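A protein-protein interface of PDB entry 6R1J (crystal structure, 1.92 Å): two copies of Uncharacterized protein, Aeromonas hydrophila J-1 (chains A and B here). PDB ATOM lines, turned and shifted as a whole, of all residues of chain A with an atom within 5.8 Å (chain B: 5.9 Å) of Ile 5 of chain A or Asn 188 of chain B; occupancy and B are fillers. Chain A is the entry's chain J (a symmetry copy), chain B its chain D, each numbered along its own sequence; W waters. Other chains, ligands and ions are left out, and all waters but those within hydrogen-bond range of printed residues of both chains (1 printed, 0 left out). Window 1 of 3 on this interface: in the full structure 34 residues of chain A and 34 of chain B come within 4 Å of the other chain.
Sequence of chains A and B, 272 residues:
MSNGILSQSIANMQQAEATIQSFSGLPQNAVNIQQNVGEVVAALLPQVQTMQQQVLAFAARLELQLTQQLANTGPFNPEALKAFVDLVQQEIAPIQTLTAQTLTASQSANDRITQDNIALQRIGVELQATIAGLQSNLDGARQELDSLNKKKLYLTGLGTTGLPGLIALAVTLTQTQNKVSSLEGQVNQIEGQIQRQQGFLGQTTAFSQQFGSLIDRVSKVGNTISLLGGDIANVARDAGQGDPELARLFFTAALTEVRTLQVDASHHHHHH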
ATOM      1  N   ASN A   3     -19.791 -12.990  20.945  1.00  0.00           N
ATOM      2  CA  ASN A   3     -21.105 -12.515  21.437  1.00  0.00           C
ATOM      3  C   ASN A   3     -22.138 -13.658  21.440  1.00  0.00           C
ATOM      4  O   ASN A   3     -22.826 -13.774  22.466  1.00  0.00           O
ATOM      5  CB  ASN A   3     -21.646 -11.322  20.635  1.00  0.00           C
ATOM      6  CG  ASN A   3     -21.271  -9.962  21.182  1.00  0.00           C
ATOM      7  OD1 ASN A   3     -21.573  -9.650  22.335  1.00  0.00           O
ATOM      8  ND2 ASN A   3     -20.695  -9.117  20.340  1.00  0.00           N
ATOM      9  N   GLY A   4     -22.307 -14.413  20.338  1.00  0.00           N
ATOM     10  CA  GLY A   4     -23.311 -15.503  20.234  1.00  0.00           C
ATOM     11  C   GLY A   4     -23.015 -16.660  21.199  1.00  0.00           C
ATOM     12  O   GLY A   4     -21.834 -16.812  21.561  1.00  0.00           O
ATOM     13  N   ILE A   5     -24.018 -17.473  21.567  1.00  0.00           N
ATOM     14  CA  ILE A   5     -23.881 -18.585  22.564  1.00  0.00           C
ATOM     15  C   ILE A   5     -22.874 -19.634  22.070  1.00  0.00           C
ATOM     16  O   ILE A   5     -22.066 -20.071  22.898  1.00  0.00           O
ATOM     17  CB  ILE A   5     -25.243 -19.201  22.955  1.00  0.00           C
ATOM     18  CG1 ILE A   5     -26.107 -18.178  23.686  1.00  0.00           C
ATOM     19  CG2 ILE A   5     -25.086 -20.438  23.829  1.00  0.00           C
ATOM     20  CD1 ILE A   5     -25.530 -17.758  25.032  1.00  0.00           C
ATOM     21  N   LEU A   6     -22.851 -19.975  20.784  1.00  0.00           N
ATOM     22  CA  LEU A   6     -21.832 -20.937  20.287  1.00  0.00           C
ATOM     23  C   LEU A   6     -20.448 -20.332  20.440  1.00  0.00           C
ATOM     24  O   LEU A   6     -19.556 -21.042  20.982  1.00  0.00           O
ATOM     25  CB  LEU A   6     -22.133 -21.352  18.848  1.00  0.00           C
ATOM     26  CG  LEU A   6     -23.352 -22.260  18.718  1.00  0.00           C
ATOM     27  CD1 LEU A   6     -23.653 -22.559  17.266  1.00  0.00           C
ATOM     28  CD2 LEU A   6     -23.180 -23.555  19.502  1.00  0.00           C
ATOM     29  N   SER A   7     -20.263 -19.087  19.991  1.00  0.00           N
ATOM     30  CA  SER A   7     -18.977 -18.364  20.044  1.00  0.00           C
ATOM     31  C   SER A   7     -18.459 -18.260  21.486  1.00  0.00           C
ATOM     32  O   SER A   7     -17.237 -18.498  21.714  1.00  0.00           O
ATOM     33  CB  SER A   7     -19.093 -16.990  19.390  1.00  0.00           C
ATOM     34  OG  SER A   7     -19.390 -17.129  18.012  1.00  0.00           O
ATOM     35  N   GLN A   8     -19.344 -17.954  22.435  1.00  0.00           N
ATOM     36  CA  GLN A   8     -18.937 -17.789  23.843  1.00  0.00           C
ATOM     37  C   GLN A   8     -18.488 -19.126  24.426  1.00  0.00           C
ATOM     38  O   GLN A   8     -17.479 -19.137  25.125  1.00  0.00           O
ATOM     39  CB  GLN A   8     -20.077 -17.219  24.667  1.00  0.00           C
ATOM     40  CG  GLN A   8     -20.271 -15.725  24.425  1.00  0.00           C
ATOM     41  CD  GLN A   8     -21.244 -15.144  25.420  1.00  0.00           C
ATOM     42  OE1 GLN A   8     -21.206 -15.491  26.603  1.00  0.00           O
ATOM     43  NE2 GLN A   8     -22.096 -14.242  24.954  1.00  0.00           N
ATOM     44  N   SER A   9     -19.280 -20.160  24.195  1.00  0.00           N
ATOM     45  CA  SER A   9     -19.060 -21.514  24.748  1.00  0.00           C
ATOM     46  C   SER A   9     -17.706 -21.993  24.241  1.00  0.00           C
ATOM     47  O   SER A   9     -16.889 -22.467  25.039  1.00  0.00           O
ATOM     48  CB  SER A   9     -20.155 -22.456  24.325  1.00  0.00           C
ATOM     49  OG  SER A   9     -21.384 -22.110  24.918  1.00  0.00           O
ATOM     50  N   ILE A  10     -17.478 -21.819  22.939  1.00  0.00           N
ATOM     51  CA  ILE A  10     -16.197 -22.201  22.306  1.00  0.00           C
ATOM     52  C   ILE A  10     -15.048 -21.459  22.975  1.00  0.00           C
ATOM     53  O   ILE A  10     -14.100 -22.134  23.397  1.00  0.00           O
ATOM     54  CB  ILE A  10     -16.264 -22.018  20.787  1.00  0.00           C
ATOM     55  CG1 ILE A  10     -17.160 -23.083  20.170  1.00  0.00           C
ATOM     56  CG2 ILE A  10     -14.875 -22.038  20.205  1.00  0.00           C
ATOM     57  CD1 ILE A  10     -17.497 -22.844  18.714  1.00  0.00           C
ATOM     58  N   ASN A  12     -14.819 -19.957  25.917  1.00  0.00           N
ATOM     59  CA  ASN A  12     -14.727 -20.354  27.339  1.00  0.00           C
ATOM     60  C   ASN A  12     -14.097 -21.748  27.437  1.00  0.00           C
ATOM     61  O   ASN A  12     -13.262 -21.945  28.323  1.00  0.00           O
ATOM     62  CB  ASN A  12     -16.092 -20.273  28.020  1.00  0.00           C
ATOM     63  CG  ASN A  12     -16.593 -18.844  28.116  1.00  0.00           C
ATOM     64  OD1 ASN A  12     -15.781 -17.936  28.164  1.00  0.00           O
ATOM     65  ND2 ASN A  12     -17.902 -18.650  28.122  1.00  0.00           N
ATOM     66  N   GLN A 209     -19.628 -27.606  31.963  1.00  0.00           N
ATOM     67  CA  GLN A 209     -20.786 -26.660  31.969  1.00  0.00           C
ATOM     68  C   GLN A 209     -20.811 -25.905  30.615  1.00  0.00           C
ATOM     69  O   GLN A 209     -21.854 -25.873  29.998  1.00  0.00           O
ATOM     70  CB  GLN A 209     -20.697 -25.750  33.202  1.00  0.00           C
ATOM     71  CG  GLN A 209     -21.871 -24.768  33.393  1.00  0.00           C
ATOM     72  CD  GLN A 209     -21.702 -23.493  32.577  1.00  0.00           C
ATOM     73  OE1 GLN A 209     -20.610 -22.946  32.441  1.00  0.00           O
ATOM     74  NE2 GLN A 209     -22.787 -23.043  31.973  1.00  0.00           N
ATOM     75  N   GLN A 210     -19.704 -25.321  30.171  1.00  0.00           N
ATOM     76  CA  GLN A 210     -19.622 -24.612  28.867  1.00  0.00           C
ATOM     77  C   GLN A 210     -19.901 -25.597  27.731  1.00  0.00           C
ATOM     78  O   GLN A 210     -20.666 -25.265  26.785  1.00  0.00           O
ATOM     79  CB  GLN A 210     -18.262 -23.945  28.727  1.00  0.00           C
ATOM     80  CG  GLN A 210     -18.011 -22.887  29.785  1.00  0.00           C
ATOM     81  CD  GLN A 210     -18.789 -21.611  29.539  1.00  0.00           C
ATOM     82  OE1 GLN A 210     -19.178 -21.334  28.402  1.00  0.00           O
ATOM     83  NE2 GLN A 210     -19.013 -20.860  30.612  1.00  0.00           N
ATOM     84  N   SER A 213     -23.561 -26.085  27.465  1.00  0.00           N
ATOM     85  CA  SER A 213     -24.250 -24.937  26.822  1.00  0.00           C
ATOM     86  C   SER A 213     -24.120 -25.089  25.305  1.00  0.00           C
ATOM     87  O   SER A 213     -25.099 -24.857  24.581  1.00  0.00           O
ATOM     88  CB  SER A 213     -23.706 -23.638  27.308  1.00  0.00           C
ATOM     89  OG  SER A 213     -24.084 -23.454  28.657  1.00  0.00           O
ATOM     90  N   LEU A 214     -22.945 -25.492  24.835  1.00  0.00           N
ATOM     91  CA  LEU A 214     -22.728 -25.760  23.391  1.00  0.00           C
ATOM     92  C   LEU A 214     -23.660 -26.876  22.909  1.00  0.00           C
ATOM     93  O   LEU A 214     -24.341 -26.693  21.867  1.00  0.00           O
ATOM     94  CB  LEU A 214     -21.246 -26.048  23.145  1.00  0.00           C
ATOM     95  CG  LEU A 214     -20.843 -26.358  21.697  1.00  0.00           C
ATOM     96  CD1 LEU A 214     -19.371 -26.002  21.474  1.00  0.00           C
ATOM     97  CD2 LEU A 214     -21.079 -27.819  21.348  1.00  0.00           C
ATOM     98  N   ARG A 217     -27.325 -25.922  22.566  1.00  0.00           N
ATOM     99  CA  ARG A 217     -27.568 -25.009  21.411  1.00  0.00           C
ATOM    100  C   ARG A 217     -27.484 -25.815  20.118  1.00  0.00           C
ATOM    101  O   ARG A 217     -28.315 -25.600  19.245  1.00  0.00           O
ATOM    102  CB  ARG A 217     -26.564 -23.857  21.373  1.00  0.00           C
ATOM    103  CG  ARG A 217     -26.785 -22.891  20.215  1.00  0.00           C
ATOM    104  CD  ARG A 217     -28.239 -22.436  20.067  1.00  0.00           C
ATOM    105  NE  ARG A 217     -28.749 -21.796  21.278  1.00  0.00           N
ATOM    106  CZ  ARG A 217     -28.783 -20.464  21.519  1.00  0.00           C
ATOM    107  NH1 ARG A 217     -29.274 -20.017  22.657  1.00  0.00           N
ATOM    108  NH2 ARG A 217     -28.376 -19.582  20.623  1.00  0.00           N
ATOM    109  N   ASP A 264     -30.337 -18.508  16.417  1.00  0.00           N
ATOM    110  CA  ASP A 264     -29.704 -19.518  17.300  1.00  0.00           C
ATOM    111  C   ASP A 264     -28.254 -19.806  16.894  1.00  0.00           C
ATOM    112  O   ASP A 264     -27.420 -20.002  17.801  1.00  0.00           O
ATOM    113  CB  ASP A 264     -30.583 -20.770  17.358  1.00  0.00           C
ATOM    114  CG  ASP A 264     -31.861 -20.520  18.156  1.00  0.00           C
ATOM    115  OD1 ASP A 264     -32.002 -19.425  18.778  1.00  0.00           O
ATOM    116  OD2 ASP A 264     -32.718 -21.405  18.174  1.00  0.00           O
ATOM    117  N   SER A 266     -26.304 -17.723  15.256  1.00  0.00           N
ATOM    118  CA  SER A 266     -25.708 -16.387  15.008  1.00  0.00           C
ATOM    119  C   SER A 266     -24.295 -16.267  15.602  1.00  0.00           C
ATOM    120  O   SER A 266     -24.079 -16.706  16.752  1.00  0.00           O
ATOM    121  CB  SER A 266     -26.606 -15.324  15.572  1.00  0.00           C
ATOM    122  OG  SER A 266     -26.104 -14.048  15.248  1.00  0.00           O
ATOM    123  N   HIS A 267     -23.372 -15.640  14.866  1.00  0.00           N
ATOM    124  CA  HIS A 267     -21.990 -15.343  15.341  1.00  0.00           C
ATOM    125  C   HIS A 267     -22.051 -14.311  16.478  1.00  0.00           C
ATOM    126  O   HIS A 267     -21.403 -14.565  17.529  1.00  0.00           O
ATOM    127  CB  HIS A 267     -21.102 -14.842  14.199  1.00  0.00           C
ATOM    128  CG  HIS A 267     -20.856 -15.860  13.146  1.00  0.00           C
ATOM    129  ND1 HIS A 267     -20.001 -16.934  13.345  1.00  0.00           N
ATOM    130  CD2 HIS A 267     -21.305 -15.958  11.879  1.00  0.00           C
ATOM    131  CE1 HIS A 267     -19.961 -17.663  12.250  1.00  0.00           C
ATOM    132  NE2 HIS A 267     -20.740 -17.085  11.333  1.00  0.00           N
ATOM    133  N   LEU B 183     -30.276 -10.561  25.551  1.00  0.00           N
ATOM    134  CA  LEU B 183     -30.252 -10.659  27.028  1.00  0.00           C
ATOM    135  C   LEU B 183     -29.523 -11.932  27.449  1.00  0.00           C
ATOM    136  O   LEU B 183     -28.703 -11.842  28.391  1.00  0.00           O
ATOM    137  CB  LEU B 183     -31.658 -10.568  27.624  1.00  0.00           C
ATOM    138  CG  LEU B 183     -32.284  -9.171  27.657  1.00  0.00           C
ATOM    139  CD1 LEU B 183     -33.768  -9.244  27.998  1.00  0.00           C
ATOM    140  CD2 LEU B 183     -31.550  -8.243  28.634  1.00  0.00           C
ATOM    141  N   GLU B 184     -29.780 -13.047  26.774  1.00  0.00           N
ATOM    142  CA  GLU B 184     -29.072 -14.327  27.060  1.00  0.00           C
ATOM    143  C   GLU B 184     -27.580 -14.131  26.878  1.00  0.00           C
ATOM    144  O   GLU B 184     -26.798 -14.597  27.732  1.00  0.00           O
ATOM    145  CB  GLU B 184     -29.342 -15.423  26.035  1.00  0.00           C
ATOM    146  CG  GLU B 184     -30.569 -16.243  26.244  1.00  0.00           C
ATOM    147  CD  GLU B 184     -30.632 -17.392  25.215  1.00  0.00           C
ATOM    148  OE1 GLU B 184     -29.809 -17.431  24.201  1.00  0.00           O
ATOM    149  OE2 GLU B 184     -31.510 -18.208  25.374  1.00  0.00           O
ATOM    150  N   GLY B 185     -27.207 -13.575  25.732  1.00  0.00           N
ATOM    151  CA  GLY B 185     -25.804 -13.327  25.380  1.00  0.00           C
ATOM    152  C   GLY B 185     -25.143 -12.474  26.451  1.00  0.00           C
ATOM    153  O   GLY B 185     -24.013 -12.774  26.834  1.00  0.00           O
ATOM    154  N   GLN B 186     -25.815 -11.408  26.902  1.00  0.00           N
ATOM    155  CA  GLN B 186     -25.284 -10.506  27.952  1.00  0.00           C
ATOM    156  C   GLN B 186     -25.125 -11.275  29.267  1.00  0.00           C
ATOM    157  O   GLN B 186     -24.074 -11.128  29.892  1.00  0.00           O
ATOM    158  CB  GLN B 186     -26.165  -9.285  28.214  1.00  0.00           C
ATOM    159  CG  GLN B 186     -26.091  -8.232  27.138  1.00  0.00           C
ATOM    160  CD  GLN B 186     -27.162  -7.191  27.378  1.00  0.00           C
ATOM    161  OE1 GLN B 186     -28.001  -6.937  26.506  1.00  0.00           O
ATOM    162  NE2 GLN B 186     -27.203  -6.663  28.595  1.00  0.00           N
ATOM    163  N   VAL B 187     -26.156 -11.991  29.717  1.00  0.00           N
ATOM    164  CA  VAL B 187     -26.107 -12.788  30.988  1.00  0.00           C
ATOM    165  C   VAL B 187     -24.990 -13.843  30.890  1.00  0.00           C
ATOM    166  O   VAL B 187     -24.178 -13.998  31.847  1.00  0.00           O
ATOM    167  CB  VAL B 187     -27.461 -13.452  31.293  1.00  0.00           C
ATOM    168  CG1 VAL B 187     -27.348 -14.537  32.373  1.00  0.00           C
ATOM    169  CG2 VAL B 187     -28.501 -12.398  31.677  1.00  0.00           C
ATOM    170  N   ASN B 188     -24.942 -14.542  29.764  1.00  0.00           N
ATOM    171  CA  ASN B 188     -23.964 -15.637  29.532  1.00  0.00           C
ATOM    172  C   ASN B 188     -22.532 -15.083  29.603  1.00  0.00           C
ATOM    173  O   ASN B 188     -21.664 -15.705  30.279  1.00  0.00           O
ATOM    174  CB  ASN B 188     -24.265 -16.347  28.221  1.00  0.00           C
ATOM    175  CG  ASN B 188     -23.646 -17.725  28.247  1.00  0.00           C
ATOM    176  OD1 ASN B 188     -24.102 -18.579  29.000  1.00  0.00           O
ATOM    177  ND2 ASN B 188     -22.564 -17.899  27.513  1.00  0.00           N
ATOM    178  N   GLN B 189     -22.313 -13.887  29.041  1.00  0.00           N
ATOM    179  CA  GLN B 189     -20.996 -13.214  29.048  1.00  0.00           C
ATOM    180  C   GLN B 189     -20.545 -12.950  30.486  1.00  0.00           C
ATOM    181  O   GLN B 189     -19.367 -13.236  30.840  1.00  0.00           O
ATOM    182  CB  GLN B 189     -21.088 -11.885  28.290  1.00  0.00           C
ATOM    183  CG  GLN B 189     -19.758 -11.163  28.200  1.00  0.00           C
ATOM    184  CD  GLN B 189     -18.751 -12.016  27.472  1.00  0.00           C
ATOM    185  OE1 GLN B 189     -19.058 -12.645  26.456  1.00  0.00           O
ATOM    186  NE2 GLN B 189     -17.533 -12.046  27.990  1.00  0.00           N
ATOM    187  N   ILE B 190     -21.421 -12.380  31.292  1.00  0.00           N
ATOM    188  CA  ILE B 190     -21.068 -12.032  32.694  1.00  0.00           C
ATOM    189  C   ILE B 190     -20.861 -13.326  33.496  1.00  0.00           C
ATOM    190  O   ILE B 190     -19.915 -13.372  34.299  1.00  0.00           O
ATOM    191  CB  ILE B 190     -22.125 -11.110  33.306  1.00  0.00           C
ATOM    192  CG1 ILE B 190     -22.252  -9.786  32.543  1.00  0.00           C
ATOM    193  CG2 ILE B 190     -21.811 -10.871  34.768  1.00  0.00           C
ATOM    194  CD1 ILE B 190     -23.528  -9.039  32.903  1.00  0.00           C
ATOM    195  N   GLU B 191     -21.681 -14.347  33.262  1.00  0.00           N
ATOM    196  CA  GLU B 191     -21.575 -15.647  33.987  1.00  0.00           C
ATOM    197  C   GLU B 191     -20.207 -16.267  33.704  1.00  0.00           C
ATOM    198  O   GLU B 191     -19.586 -16.759  34.684  1.00  0.00           O
ATOM    199  CB  GLU B 191     -22.715 -16.607  33.638  1.00  0.00           C
ATOM    200  CG  GLU B 191     -23.986 -16.252  34.367  1.00  0.00           C
ATOM    201  CD  GLU B 191     -25.209 -17.108  34.083  1.00  0.00           C
ATOM    202  OE1 GLU B 191     -25.204 -17.857  33.064  1.00  0.00           O
ATOM    203  OE2 GLU B 191     -26.169 -17.017  34.893  1.00  0.00           O
ATOM    204  N   GLY B 192     -19.759 -16.194  32.451  1.00  0.00           N
ATOM    205  CA  GLY B 192     -18.440 -16.674  31.973  1.00  0.00           C
ATOM    206  C   GLY B 192     -17.306 -15.988  32.714  1.00  0.00           C
ATOM    207  O   GLY B 192     -16.378 -16.695  33.146  1.00  0.00           O
ATOM    208  N   GLN B 193     -17.384 -14.663  32.868  1.00  0.00           N
ATOM    209  CA  GLN B 193     -16.406 -13.820  33.602  1.00  0.00           C
ATOM    210  C   GLN B 193     -16.340 -14.258  35.078  1.00  0.00           C
ATOM    211  O   GLN B 193     -15.234 -14.424  35.631  1.00  0.00           O
ATOM    212  CB  GLN B 193     -16.821 -12.337  33.499  1.00  0.00           C
ATOM    213  CG  GLN B 193     -16.845 -11.798  32.066  1.00  0.00           C
ATOM    214  CD  GLN B 193     -17.226 -10.344  31.875  1.00  0.00           C
ATOM    215  OE1 GLN B 193     -18.261  -9.844  32.323  1.00  0.00           O
ATOM    216  NE2 GLN B 193     -16.410  -9.658  31.110  1.00  0.00           N
HETATM  217  O   HOH W   1     -21.468 -20.622  27.360  1.00  0.00           O
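NH1 of Arg 217 of chain A lies within salt-bridge range of OE1 of Glu 184 of chain B, 3.1 Å away.
The side-chain amide oxygen (OE1) of Gln 8 of chain A is in hydrogen-bond range of the side-chain amide nitrogen (ND2) of Asn 188 of chain B (2.9 Å).
The backbone carbonyl oxygen (O) of Gly 185 of chain B lies within hydrogen-bond range of the side-chain amide nitrogen (NE2) of Gln 8 of chain A (3.1 Å).
N of Gln 189 of chain B lies within hydrogen-bond range of OE1 of Gln 8 of chain A, at 3.1 Å.
NE2 of Gln 8 of chain A sits at hydrogen-bond distance from O of Asn 3 of chain A.
The backbone carbonyl oxygen (O) of Gln 8 of chain A lies within hydrogen-bond range of the side-chain amide nitrogen (ND2) of Asn 12 of chain A (3.1 Å).
OG of Ser 9 of chain A lies within hydrogen-bond range of O of Ile 5 of chain A.
NH2 of Arg 217 of chain A is in hydrogen-bond range of O of Asp 264 of chain A, at 3.0 Å.
Among the printed residues, pairs that only touch across the chains: Ile 5 of chain A with Asn 188 of chain B and Ile 5 of chain A with Glu 184 of chain B.
Ile 5 of chain A touches just these residues of chain B: Glu 184 (3.8 Å) and Asn 188 (3.7 Å).
Of the printed residues of chain B, Gln 8 of chain A touches Gly 185 (3.1 Å), Asn 188 (2.9 Å) and Gln 189 (3.1 Å).
Of the printed residues of chain B, Arg 217 of chain A touches Glu 184 (3.1 Å).
Of the printed residues of chain A, Glu 184 of chain B touches Ile 5 and Arg 217.
Of the printed residues of chain A, Gly 185 of chain B touches Gln 8.
Asn 188 of chain B touches just these residues of chain A: Ile 5 and Gln 8.
The nearest residue of chain B that does not touch Ile 5 of chain A is Gly 185 of chain B (4.5 Å).
Of the 17 printed residues of chain A, 3 touch a printed residue of chain B.
Hydrophobic or aromatic side chains of chain A that line the printed part of chain B: Ile 5.
Along chain A the printed residues that touch a printed residue of chain B span positions 5 to 217.
Along chain B the printed residues that touch a printed residue of chain A span positions 184 to 189.
No position is printed for both chains.
Of the 6 pairs that touch across the chains among the printed residues, none has its exchanged pair printed and touching as well.
Water W1 lies within hydrogen-bond range of the side-chain amide oxygen of Gln 210 of chain A (2.6 Å), the side-chain hydroxyl of Ser 9 of chain A (2.9 Å) and the side-chain amide nitrogen of Asn 188 of chain B (2.9 Å).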
